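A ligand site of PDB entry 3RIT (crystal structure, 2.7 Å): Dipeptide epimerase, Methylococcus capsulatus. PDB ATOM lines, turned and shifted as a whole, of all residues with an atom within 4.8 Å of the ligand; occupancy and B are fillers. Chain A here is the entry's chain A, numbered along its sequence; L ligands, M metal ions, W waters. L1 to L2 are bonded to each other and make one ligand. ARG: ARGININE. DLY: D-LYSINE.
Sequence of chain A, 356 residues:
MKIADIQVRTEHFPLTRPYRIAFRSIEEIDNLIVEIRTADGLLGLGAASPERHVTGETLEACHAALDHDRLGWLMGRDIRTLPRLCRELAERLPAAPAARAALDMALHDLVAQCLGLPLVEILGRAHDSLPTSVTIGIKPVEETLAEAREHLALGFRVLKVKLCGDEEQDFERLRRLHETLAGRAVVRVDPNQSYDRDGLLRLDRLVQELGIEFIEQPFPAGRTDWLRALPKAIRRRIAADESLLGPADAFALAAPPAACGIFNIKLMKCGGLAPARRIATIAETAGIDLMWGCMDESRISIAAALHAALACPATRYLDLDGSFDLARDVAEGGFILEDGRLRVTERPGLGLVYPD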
ATOM      1  N   LEU A  15     -21.553  16.122  16.397  1.00  0.00           N
ATOM      2  CA  LEU A  15     -22.541  17.184  16.514  1.00  0.00           C
ATOM      3  C   LEU A  15     -23.851  16.661  17.122  1.00  0.00           C
ATOM      4  O   LEU A  15     -24.293  15.566  16.787  1.00  0.00           O
ATOM      5  CB  LEU A  15     -22.841  17.802  15.159  1.00  0.00           C
ATOM      6  CG  LEU A  15     -21.719  18.473  14.368  1.00  0.00           C
ATOM      7  CD1 LEU A  15     -22.309  19.510  13.413  1.00  0.00           C
ATOM      8  CD2 LEU A  15     -20.681  19.117  15.279  1.00  0.00           C
ATOM      9  N   TYR A  19     -26.062  19.048   9.869  1.00  0.00           N
ATOM     10  CA  TYR A  19     -26.643  20.077   9.000  1.00  0.00           C
ATOM     11  C   TYR A  19     -26.010  20.060   7.600  1.00  0.00           C
ATOM     12  O   TYR A  19     -24.933  19.493   7.422  1.00  0.00           O
ATOM     13  CB  TYR A  19     -26.500  21.471   9.641  1.00  0.00           C
ATOM     14  CG  TYR A  19     -25.074  22.010   9.723  1.00  0.00           C
ATOM     15  CD1 TYR A  19     -24.144  21.465  10.617  1.00  0.00           C
ATOM     16  CD2 TYR A  19     -24.669  23.072   8.925  1.00  0.00           C
ATOM     17  CE1 TYR A  19     -22.839  21.951  10.697  1.00  0.00           C
ATOM     18  CE2 TYR A  19     -23.384  23.563   8.991  1.00  0.00           C
ATOM     19  CZ  TYR A  19     -22.468  23.006   9.873  1.00  0.00           C
ATOM     20  OH  TYR A  19     -21.188  23.518   9.915  1.00  0.00           O
ATOM     21  N   ILE A  21     -24.674  22.194   4.103  1.00  0.00           N
ATOM     22  CA  ILE A  21     -24.268  23.447   3.477  1.00  0.00           C
ATOM     23  C   ILE A  21     -24.294  23.169   1.991  1.00  0.00           C
ATOM     24  O   ILE A  21     -24.281  21.993   1.589  1.00  0.00           O
ATOM     25  CB  ILE A  21     -22.842  23.865   3.863  1.00  0.00           C
ATOM     26  CG1 ILE A  21     -22.237  22.873   4.856  1.00  0.00           C
ATOM     27  CG2 ILE A  21     -22.830  25.282   4.417  1.00  0.00           C
ATOM     28  CD1 ILE A  21     -20.770  23.125   5.135  1.00  0.00           C
ATOM     29  N   ARG A  24     -22.194  20.357   0.538  1.00  0.00           N
ATOM     30  CA  ARG A  24     -21.374  19.715   1.591  1.00  0.00           C
ATOM     31  C   ARG A  24     -21.920  18.656   2.617  1.00  0.00           C
ATOM     32  O   ARG A  24     -21.479  17.516   2.552  1.00  0.00           O
ATOM     33  CB  ARG A  24     -20.445  20.736   2.256  1.00  0.00           C
ATOM     34  CG  ARG A  24     -19.306  21.201   1.336  1.00  0.00           C
ATOM     35  CD  ARG A  24     -17.934  20.730   1.807  1.00  0.00           C
ATOM     36  NE  ARG A  24     -17.589  21.305   3.104  1.00  0.00           N
ATOM     37  CZ  ARG A  24     -17.313  20.597   4.193  1.00  0.00           C
ATOM     38  NH1 ARG A  24     -17.307  19.267   4.170  1.00  0.00           N
ATOM     39  NH2 ARG A  24     -17.037  21.234   5.331  1.00  0.00           N
ATOM     40  N   GLU A  51     -10.190  24.056   7.287  1.00  0.00           N
ATOM     41  CA  GLU A  51     -11.250  23.952   6.287  1.00  0.00           C
ATOM     42  C   GLU A  51     -10.618  23.765   4.898  1.00  0.00           C
ATOM     43  O   GLU A  51     -10.204  24.740   4.265  1.00  0.00           O
ATOM     44  CB  GLU A  51     -12.071  25.253   6.343  1.00  0.00           C
ATOM     45  CG  GLU A  51     -13.304  25.295   5.444  1.00  0.00           C
ATOM     46  CD  GLU A  51     -14.182  24.072   5.594  1.00  0.00           C
ATOM     47  OE1 GLU A  51     -14.605  23.771   6.743  1.00  0.00           O
ATOM     48  OE2 GLU A  51     -14.438  23.390   4.566  1.00  0.00           O
ATOM     49  N   VAL A  54     -11.855  25.763   1.561  1.00  0.00           N
ATOM     50  CA  VAL A  54     -11.502  27.168   1.578  1.00  0.00           C
ATOM     51  C   VAL A  54      -9.995  27.471   1.572  1.00  0.00           C
ATOM     52  O   VAL A  54      -9.538  28.294   0.781  1.00  0.00           O
ATOM     53  CB  VAL A  54     -12.148  27.870   2.759  1.00  0.00           C
ATOM     54  CG1 VAL A  54     -11.879  29.350   2.687  1.00  0.00           C
ATOM     55  CG2 VAL A  54     -13.647  27.560   2.786  1.00  0.00           C
ATOM     56  N   THR A 135     -27.101  29.259  13.272  1.00  0.00           N
ATOM     57  CA  THR A 135     -27.187  28.847  11.887  1.00  0.00           C
ATOM     58  C   THR A 135     -28.277  27.819  11.630  1.00  0.00           C
ATOM     59  O   THR A 135     -28.416  26.845  12.348  1.00  0.00           O
ATOM     60  CB  THR A 135     -25.834  28.283  11.387  1.00  0.00           C
ATOM     61  OG1 THR A 135     -24.806  29.253  11.625  1.00  0.00           O
ATOM     62  CG2 THR A 135     -25.886  27.955   9.921  1.00  0.00           C
ATOM     63  N   LYS A 160     -28.923  33.045  10.952  1.00  0.00           N
ATOM     64  CA  LYS A 160     -28.189  32.971   9.710  1.00  0.00           C
ATOM     65  C   LYS A 160     -28.709  31.794   8.911  1.00  0.00           C
ATOM     66  O   LYS A 160     -28.587  30.636   9.327  1.00  0.00           O
ATOM     67  CB  LYS A 160     -26.697  32.798   9.988  1.00  0.00           C
ATOM     68  CG  LYS A 160     -25.882  32.477   8.753  1.00  0.00           C
ATOM     69  CD  LYS A 160     -24.483  33.064   8.852  1.00  0.00           C
ATOM     70  CE  LYS A 160     -23.467  32.169   8.204  1.00  0.00           C
ATOM     71  NZ  LYS A 160     -22.180  32.857   7.987  1.00  0.00           N
ATOM     72  N   LYS A 162     -28.808  29.387   5.593  1.00  0.00           N
ATOM     73  CA  LYS A 162     -28.111  28.885   4.410  1.00  0.00           C
ATOM     74  C   LYS A 162     -29.073  28.774   3.235  1.00  0.00           C
ATOM     75  O   LYS A 162     -30.124  28.144   3.356  1.00  0.00           O
ATOM     76  CB  LYS A 162     -27.517  27.505   4.681  1.00  0.00           C
ATOM     77  CG  LYS A 162     -26.523  27.452   5.814  1.00  0.00           C
ATOM     78  CD  LYS A 162     -25.253  28.132   5.421  1.00  0.00           C
ATOM     79  CE  LYS A 162     -24.142  27.861   6.398  1.00  0.00           C
ATOM     80  NZ  LYS A 162     -22.933  28.491   5.864  1.00  0.00           N
ATOM     81  N   ASP A 190     -26.891  33.284   3.615  1.00  0.00           N
ATOM     82  CA  ASP A 190     -25.598  32.795   3.146  1.00  0.00           C
ATOM     83  C   ASP A 190     -25.702  31.728   2.036  1.00  0.00           C
ATOM     84  O   ASP A 190     -25.742  30.531   2.322  1.00  0.00           O
ATOM     85  CB  ASP A 190     -24.784  32.291   4.342  1.00  0.00           C
ATOM     86  CG  ASP A 190     -23.425  31.774   3.943  1.00  0.00           C
ATOM     87  OD1 ASP A 190     -23.090  31.894   2.739  1.00  0.00           O
ATOM     88  OD2 ASP A 190     -22.704  31.262   4.831  1.00  0.00           O
ATOM     89  N   ASN A 192     -23.570  30.860  -0.092  1.00  0.00           N
ATOM     90  CA  ASN A 192     -22.318  30.151  -0.316  1.00  0.00           C
ATOM     91  C   ASN A 192     -21.945  29.909  -1.778  1.00  0.00           C
ATOM     92  O   ASN A 192     -21.797  28.760  -2.168  1.00  0.00           O
ATOM     93  CB  ASN A 192     -22.364  28.803   0.378  1.00  0.00           C
ATOM     94  CG  ASN A 192     -21.216  28.623   1.281  1.00  0.00           C
ATOM     95  OD1 ASN A 192     -21.373  28.667   2.509  1.00  0.00           O
ATOM     96  ND2 ASN A 192     -20.024  28.493   0.695  1.00  0.00           N
ATOM     97  N   GLU A 216     -24.308  36.975   2.377  1.00  0.00           N
ATOM     98  CA  GLU A 216     -22.943  36.505   2.514  1.00  0.00           C
ATOM     99  C   GLU A 216     -22.489  35.694   1.297  1.00  0.00           C
ATOM    100  O   GLU A 216     -23.120  34.698   0.934  1.00  0.00           O
ATOM    101  CB  GLU A 216     -22.812  35.684   3.793  1.00  0.00           C
ATOM    102  CG  GLU A 216     -21.404  35.372   4.125  1.00  0.00           C
ATOM    103  CD  GLU A 216     -21.286  34.577   5.395  1.00  0.00           C
ATOM    104  OE1 GLU A 216     -22.208  34.683   6.224  1.00  0.00           O
ATOM    105  OE2 GLU A 216     -20.283  33.850   5.563  1.00  0.00           O
ATOM    106  N   ASP A 241     -16.804  36.089   2.302  1.00  0.00           N
ATOM    107  CA  ASP A 241     -16.294  35.036   3.164  1.00  0.00           C
ATOM    108  C   ASP A 241     -15.201  34.222   2.453  1.00  0.00           C
ATOM    109  O   ASP A 241     -14.019  34.438   2.695  1.00  0.00           O
ATOM    110  CB  ASP A 241     -17.419  34.139   3.678  1.00  0.00           C
ATOM    111  CG  ASP A 241     -16.940  33.047   4.631  1.00  0.00           C
ATOM    112  OD1 ASP A 241     -15.748  33.049   4.979  1.00  0.00           O
ATOM    113  OD2 ASP A 241     -17.758  32.203   5.059  1.00  0.00           O
ATOM    114  N   GLU A 242     -15.604  33.325   1.562  1.00  0.00           N
ATOM    115  CA  GLU A 242     -14.640  32.430   0.903  1.00  0.00           C
ATOM    116  C   GLU A 242     -13.649  33.227   0.014  1.00  0.00           C
ATOM    117  O   GLU A 242     -12.567  32.754  -0.295  1.00  0.00           O
ATOM    118  CB  GLU A 242     -15.370  31.354   0.097  1.00  0.00           C
ATOM    119  CG  GLU A 242     -16.024  30.230   0.922  1.00  0.00           C
ATOM    120  CD  GLU A 242     -17.383  30.595   1.550  1.00  0.00           C
ATOM    121  OE1 GLU A 242     -17.848  31.745   1.374  1.00  0.00           O
ATOM    122  OE2 GLU A 242     -17.980  29.735   2.231  1.00  0.00           O
ATOM    123  N   ASN A 264     -16.034  38.846   6.366  1.00  0.00           N
ATOM    124  CA  ASN A 264     -16.215  37.820   7.355  1.00  0.00           C
ATOM    125  C   ASN A 264     -14.834  37.250   7.701  1.00  0.00           C
ATOM    126  O   ASN A 264     -14.267  36.501   6.927  1.00  0.00           O
ATOM    127  CB  ASN A 264     -17.139  36.737   6.810  1.00  0.00           C
ATOM    128  CG  ASN A 264     -17.425  35.640   7.811  1.00  0.00           C
ATOM    129  OD1 ASN A 264     -16.761  35.542   8.839  1.00  0.00           O
ATOM    130  ND2 ASN A 264     -18.426  34.797   7.524  1.00  0.00           N
ATOM    131  N   LYS A 266     -12.280  34.863   9.782  1.00  0.00           N
ATOM    132  CA  LYS A 266     -12.220  33.616  10.538  1.00  0.00           C
ATOM    133  C   LYS A 266     -10.761  33.269  10.829  1.00  0.00           C
ATOM    134  O   LYS A 266      -9.943  33.171   9.919  1.00  0.00           O
ATOM    135  CB  LYS A 266     -12.877  32.463   9.779  1.00  0.00           C
ATOM    136  CG  LYS A 266     -14.319  32.709   9.363  1.00  0.00           C
ATOM    137  CD  LYS A 266     -14.918  31.430   8.763  1.00  0.00           C
ATOM    138  CE  LYS A 266     -16.159  31.744   7.930  1.00  0.00           C
ATOM    139  NZ  LYS A 266     -16.923  30.521   7.568  1.00  0.00           N
ATOM    140  N   CYS A 294     -16.879  31.627  11.895  1.00  0.00           N
ATOM    141  CA  CYS A 294     -16.200  30.437  12.406  1.00  0.00           C
ATOM    142  C   CYS A 294     -16.561  29.158  11.665  1.00  0.00           C
ATOM    143  O   CYS A 294     -17.443  29.148  10.802  1.00  0.00           O
ATOM    144  CB  CYS A 294     -16.539  30.246  13.888  1.00  0.00           C
ATOM    145  SG  CYS A 294     -18.315  29.903  14.176  1.00  0.00           S
ATOM    146  N   MET A 295     -15.868  28.090  12.055  1.00  0.00           N
ATOM    147  CA  MET A 295     -16.166  26.718  11.641  1.00  0.00           C
ATOM    148  C   MET A 295     -16.824  26.031  12.813  1.00  0.00           C
ATOM    149  O   MET A 295     -17.147  26.672  13.812  1.00  0.00           O
ATOM    150  CB  MET A 295     -14.869  25.961  11.312  1.00  0.00           C
ATOM    151  CG  MET A 295     -13.877  26.692  10.437  1.00  0.00           C
ATOM    152  SD  MET A 295     -14.559  27.176   8.845  1.00  0.00           S
ATOM    153  CE  MET A 295     -13.231  28.225   8.262  1.00  0.00           C
ATOM    154  N   ASP A 296     -17.032  24.727  12.700  1.00  0.00           N
ATOM    155  CA  ASP A 296     -17.333  23.939  13.885  1.00  0.00           C
ATOM    156  C   ASP A 296     -16.053  23.851  14.707  1.00  0.00           C
ATOM    157  O   ASP A 296     -15.031  23.368  14.223  1.00  0.00           O
ATOM    158  CB  ASP A 296     -17.880  22.577  13.475  1.00  0.00           C
ATOM    159  CG  ASP A 296     -19.183  22.686  12.702  1.00  0.00           C
ATOM    160  OD1 ASP A 296     -20.252  22.771  13.356  1.00  0.00           O
ATOM    161  OD2 ASP A 296     -19.157  22.694  11.447  1.00  0.00           O
ATOM    162  N   ASP A 319     -20.758  35.953  13.974  1.00  0.00           N
ATOM    163  CA  ASP A 319     -21.356  34.647  13.776  1.00  0.00           C
ATOM    164  C   ASP A 319     -20.429  33.636  14.440  1.00  0.00           C
ATOM    165  O   ASP A 319     -19.626  32.964  13.802  1.00  0.00           O
ATOM    166  CB  ASP A 319     -21.510  34.429  12.283  1.00  0.00           C
ATOM    167  CG  ASP A 319     -22.101  33.089  11.945  1.00  0.00           C
ATOM    168  OD1 ASP A 319     -22.996  32.611  12.689  1.00  0.00           O
ATOM    169  OD2 ASP A 319     -21.685  32.513  10.913  1.00  0.00           O
ATOM    170  N   ASP A 321     -21.414  30.841  16.583  1.00  0.00           N
ATOM    171  CA  ASP A 321     -22.149  29.683  17.096  1.00  0.00           C
ATOM    172  C   ASP A 321     -21.429  28.338  16.908  1.00  0.00           C
ATOM    173  O   ASP A 321     -22.047  27.280  17.062  1.00  0.00           O
ATOM    174  CB  ASP A 321     -23.524  29.619  16.443  1.00  0.00           C
ATOM    175  CG  ASP A 321     -23.467  29.307  14.949  1.00  0.00           C
ATOM    176  OD1 ASP A 321     -22.390  29.447  14.328  1.00  0.00           O
ATOM    177  OD2 ASP A 321     -24.525  28.941  14.388  1.00  0.00           O
ATOM    178  N   GLY A 322     -20.171  28.372  16.502  1.00  0.00           N
ATOM    179  CA  GLY A 322     -19.455  27.162  16.123  1.00  0.00           C
ATOM    180  C   GLY A 322     -19.283  26.087  17.176  1.00  0.00           C
ATOM    181  O   GLY A 322     -19.066  24.919  16.862  1.00  0.00           O
ATOM    182  N   ASP A 325     -23.293  23.421  19.035  1.00  0.00           N
ATOM    183  CA  ASP A 325     -23.862  22.118  18.678  1.00  0.00           C
ATOM    184  C   ASP A 325     -22.888  20.956  18.878  1.00  0.00           C
ATOM    185  O   ASP A 325     -23.173  19.829  18.488  1.00  0.00           O
ATOM    186  CB  ASP A 325     -24.467  22.130  17.265  1.00  0.00           C
ATOM    187  CG  ASP A 325     -25.643  23.140  17.148  1.00  0.00           C
ATOM    188  OD1 ASP A 325     -26.143  23.611  18.196  1.00  0.00           O
ATOM    189  OD2 ASP A 325     -26.084  23.455  16.016  1.00  0.00           O
HETATM  190  N   ARG L   1     -21.197  29.714  11.618  1.00  0.00           N
HETATM  191  CA  ARG L   1     -20.656  29.184  10.368  1.00  0.00           C
HETATM  192  C   ARG L   1     -21.781  29.211   9.365  1.00  0.00           C
HETATM  193  O   ARG L   1     -22.921  29.284   9.790  1.00  0.00           O
HETATM  194  CB  ARG L   1     -20.184  27.753  10.572  1.00  0.00           C
HETATM  195  CG  ARG L   1     -20.488  27.181  11.935  1.00  0.00           C
HETATM  196  CD  ARG L   1     -21.913  26.699  12.025  1.00  0.00           C
HETATM  197  NE  ARG L   1     -21.986  25.553  12.920  1.00  0.00           N
HETATM  198  CZ  ARG L   1     -23.067  24.789  13.085  1.00  0.00           C
HETATM  199  NH1 ARG L   1     -24.174  25.051  12.421  1.00  0.00           N
HETATM  200  NH2 ARG L   1     -23.032  23.760  13.927  1.00  0.00           N
HETATM  201  N   DLY L   2     -21.518  29.177   8.052  1.00  0.00           N
HETATM  202  CA  DLY L   2     -20.172  29.106   7.417  1.00  0.00           C
HETATM  203  C   DLY L   2     -20.062  30.056   6.226  1.00  0.00           C
HETATM  204  O   DLY L   2     -20.294  31.290   6.370  1.00  0.00           O
HETATM  205  CB  DLY L   2     -19.979  27.673   6.882  1.00  0.00           C
HETATM  206  CG  DLY L   2     -19.137  26.744   7.770  1.00  0.00           C
HETATM  207  CD  DLY L   2     -18.186  25.886   6.944  1.00  0.00           C
HETATM  208  CE  DLY L   2     -17.328  26.732   6.001  1.00  0.00           C
HETATM  209  NZ  DLY L   2     -17.000  25.985   4.806  1.00  0.00           N
HETATM  210  OXT DLY L   2     -19.734  29.576   5.097  1.00  0.00           O
HETATM  211 MG    MG M   1     -20.213  32.245   3.373  1.00  0.00          MG
HETATM  212  O   HOH W   1     -21.033  23.323  16.133  1.00  0.00           O
HETATM  213  O   HOH W   2     -23.595  25.262  16.112  1.00  0.00           O
HETATM  214  O   HOH W   3     -26.011  22.497  13.440  1.00  0.00           O
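The side-chain amino group (NZ) of Lys 162 is in salt-bridge range of the side-chain carboxylate (OD2) of Asp 190, 3.0 Å away.
OD2 of Asp 190 is in salt-bridge range of NZ of Lys 160 (3.6 Å).
The backbone NH of Asn 192 sits at hydrogen-bond distance from the side-chain carboxylate of Asp 190 (3.1 Å).
The backbone carbonyl oxygen (O) of Asp 319 sits at hydrogen-bond distance from the side-chain sulfur (SG) of Cys 294, 3.4 Å away.
The side-chain carboxylate (OD2) of Asp 241 is in salt-bridge range of the side-chain amino group (NZ) of Lys 266, 3.1 Å away.
OD2 of Asp 296 lies within hydrogen-bond range of OH of Tyr 19.
N of Gly 322 sits at hydrogen-bond distance from SG of Cys 294 (3.3 Å).
ND2 of Asn 192 lies within hydrogen-bond range of OE2 of Glu 242, at 2.8 Å.
OG1 of Thr 135 is in hydrogen-bond range of O of ARG L1, at 2.6 Å.
The side-chain carboxylate (OE2) of Glu 216 sits close to an oxygen (O) of DLY L2 (2.7 Å).
The side-chain amino group (NZ) of Lys 162 is in salt-bridge range of an oxygen (OXT) of DLY L2.
OD2 of Asp 190 sits close to O of DLY L2, at 2.9 Å.
The side-chain carboxylate of Asp 319 lies within salt-bridge range of a nitrogen (N) of ARG L1 (2.9 Å).
The side-chain amino group (NZ) of Lys 160 lies within salt-bridge range of an oxygen (O) of DLY L2 (2.9 Å).
OD1 of Asp 321 lies within salt-bridge range of N of ARG L1, at 3.0 Å.
The side-chain carboxylate of Asp 241 sits close to an oxygen (O) of DLY L2 (3.0 Å).
A nitrogen (NH2) of ARG L1 is in salt-bridge range of the side-chain carboxylate (OD1) of Asp 296, at 3.0 Å.
OD1 of Asn 192 lies close to OXT of DLY L2, 3.2 Å away.
An oxygen (O) of DLY L2 is in salt-bridge range of the side-chain amino group of Lys 266 (3.7 Å).
NZ of DLY L2 lies within salt-bridge range of OE2 of Glu 51 (3.7 Å).
A nitrogen (NH2) of ARG L1 is in salt-bridge range of the side-chain carboxylate (OD2) of Asp 325, 3.7 Å away.
Water W2 lies within hydrogen-bond range of a nitrogen (NH2) of ARG L1 (2.7 Å), the backbone carbonyl oxygen of Asp 321 (2.7 Å) and the side-chain carboxylate of Asp 325 (3.1 Å).
Water W1 lies within hydrogen-bond range of the backbone carbonyl oxygen (O) of Gly 322 (2.6 Å), the side-chain carboxylate (OD1) of Asp 296 (2.9 Å) and a nitrogen (NH2) of ARG L1 (3.0 Å).
Water W3 bridges OD2 of Asp 325 (2.7 Å) and NH2 of ARG L1 (3.3 Å).
The side-chain carboxylate (OE2) of Glu 242 lies close to an oxygen (OXT) of DLY L2, at 3.4 Å.
CZ of Tyr 19 touches NH1 of ARG L1, 3.7 Å away.
O of Cys 294 touches CB of ARG L1, 3.1 Å away.
O of Met 295 touches CG of ARG L1, at 3.9 Å.
Within 4 Å of the ligand: Tyr 19, Glu 51, Thr 135, Lys 160, Lys 162, Asp 190, Asn 192, Glu 216, Asp 241, Glu 242, Lys 266, Cys 294, Met 295, Asp 296, Asp 319, Asp 321 and Asp 325.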
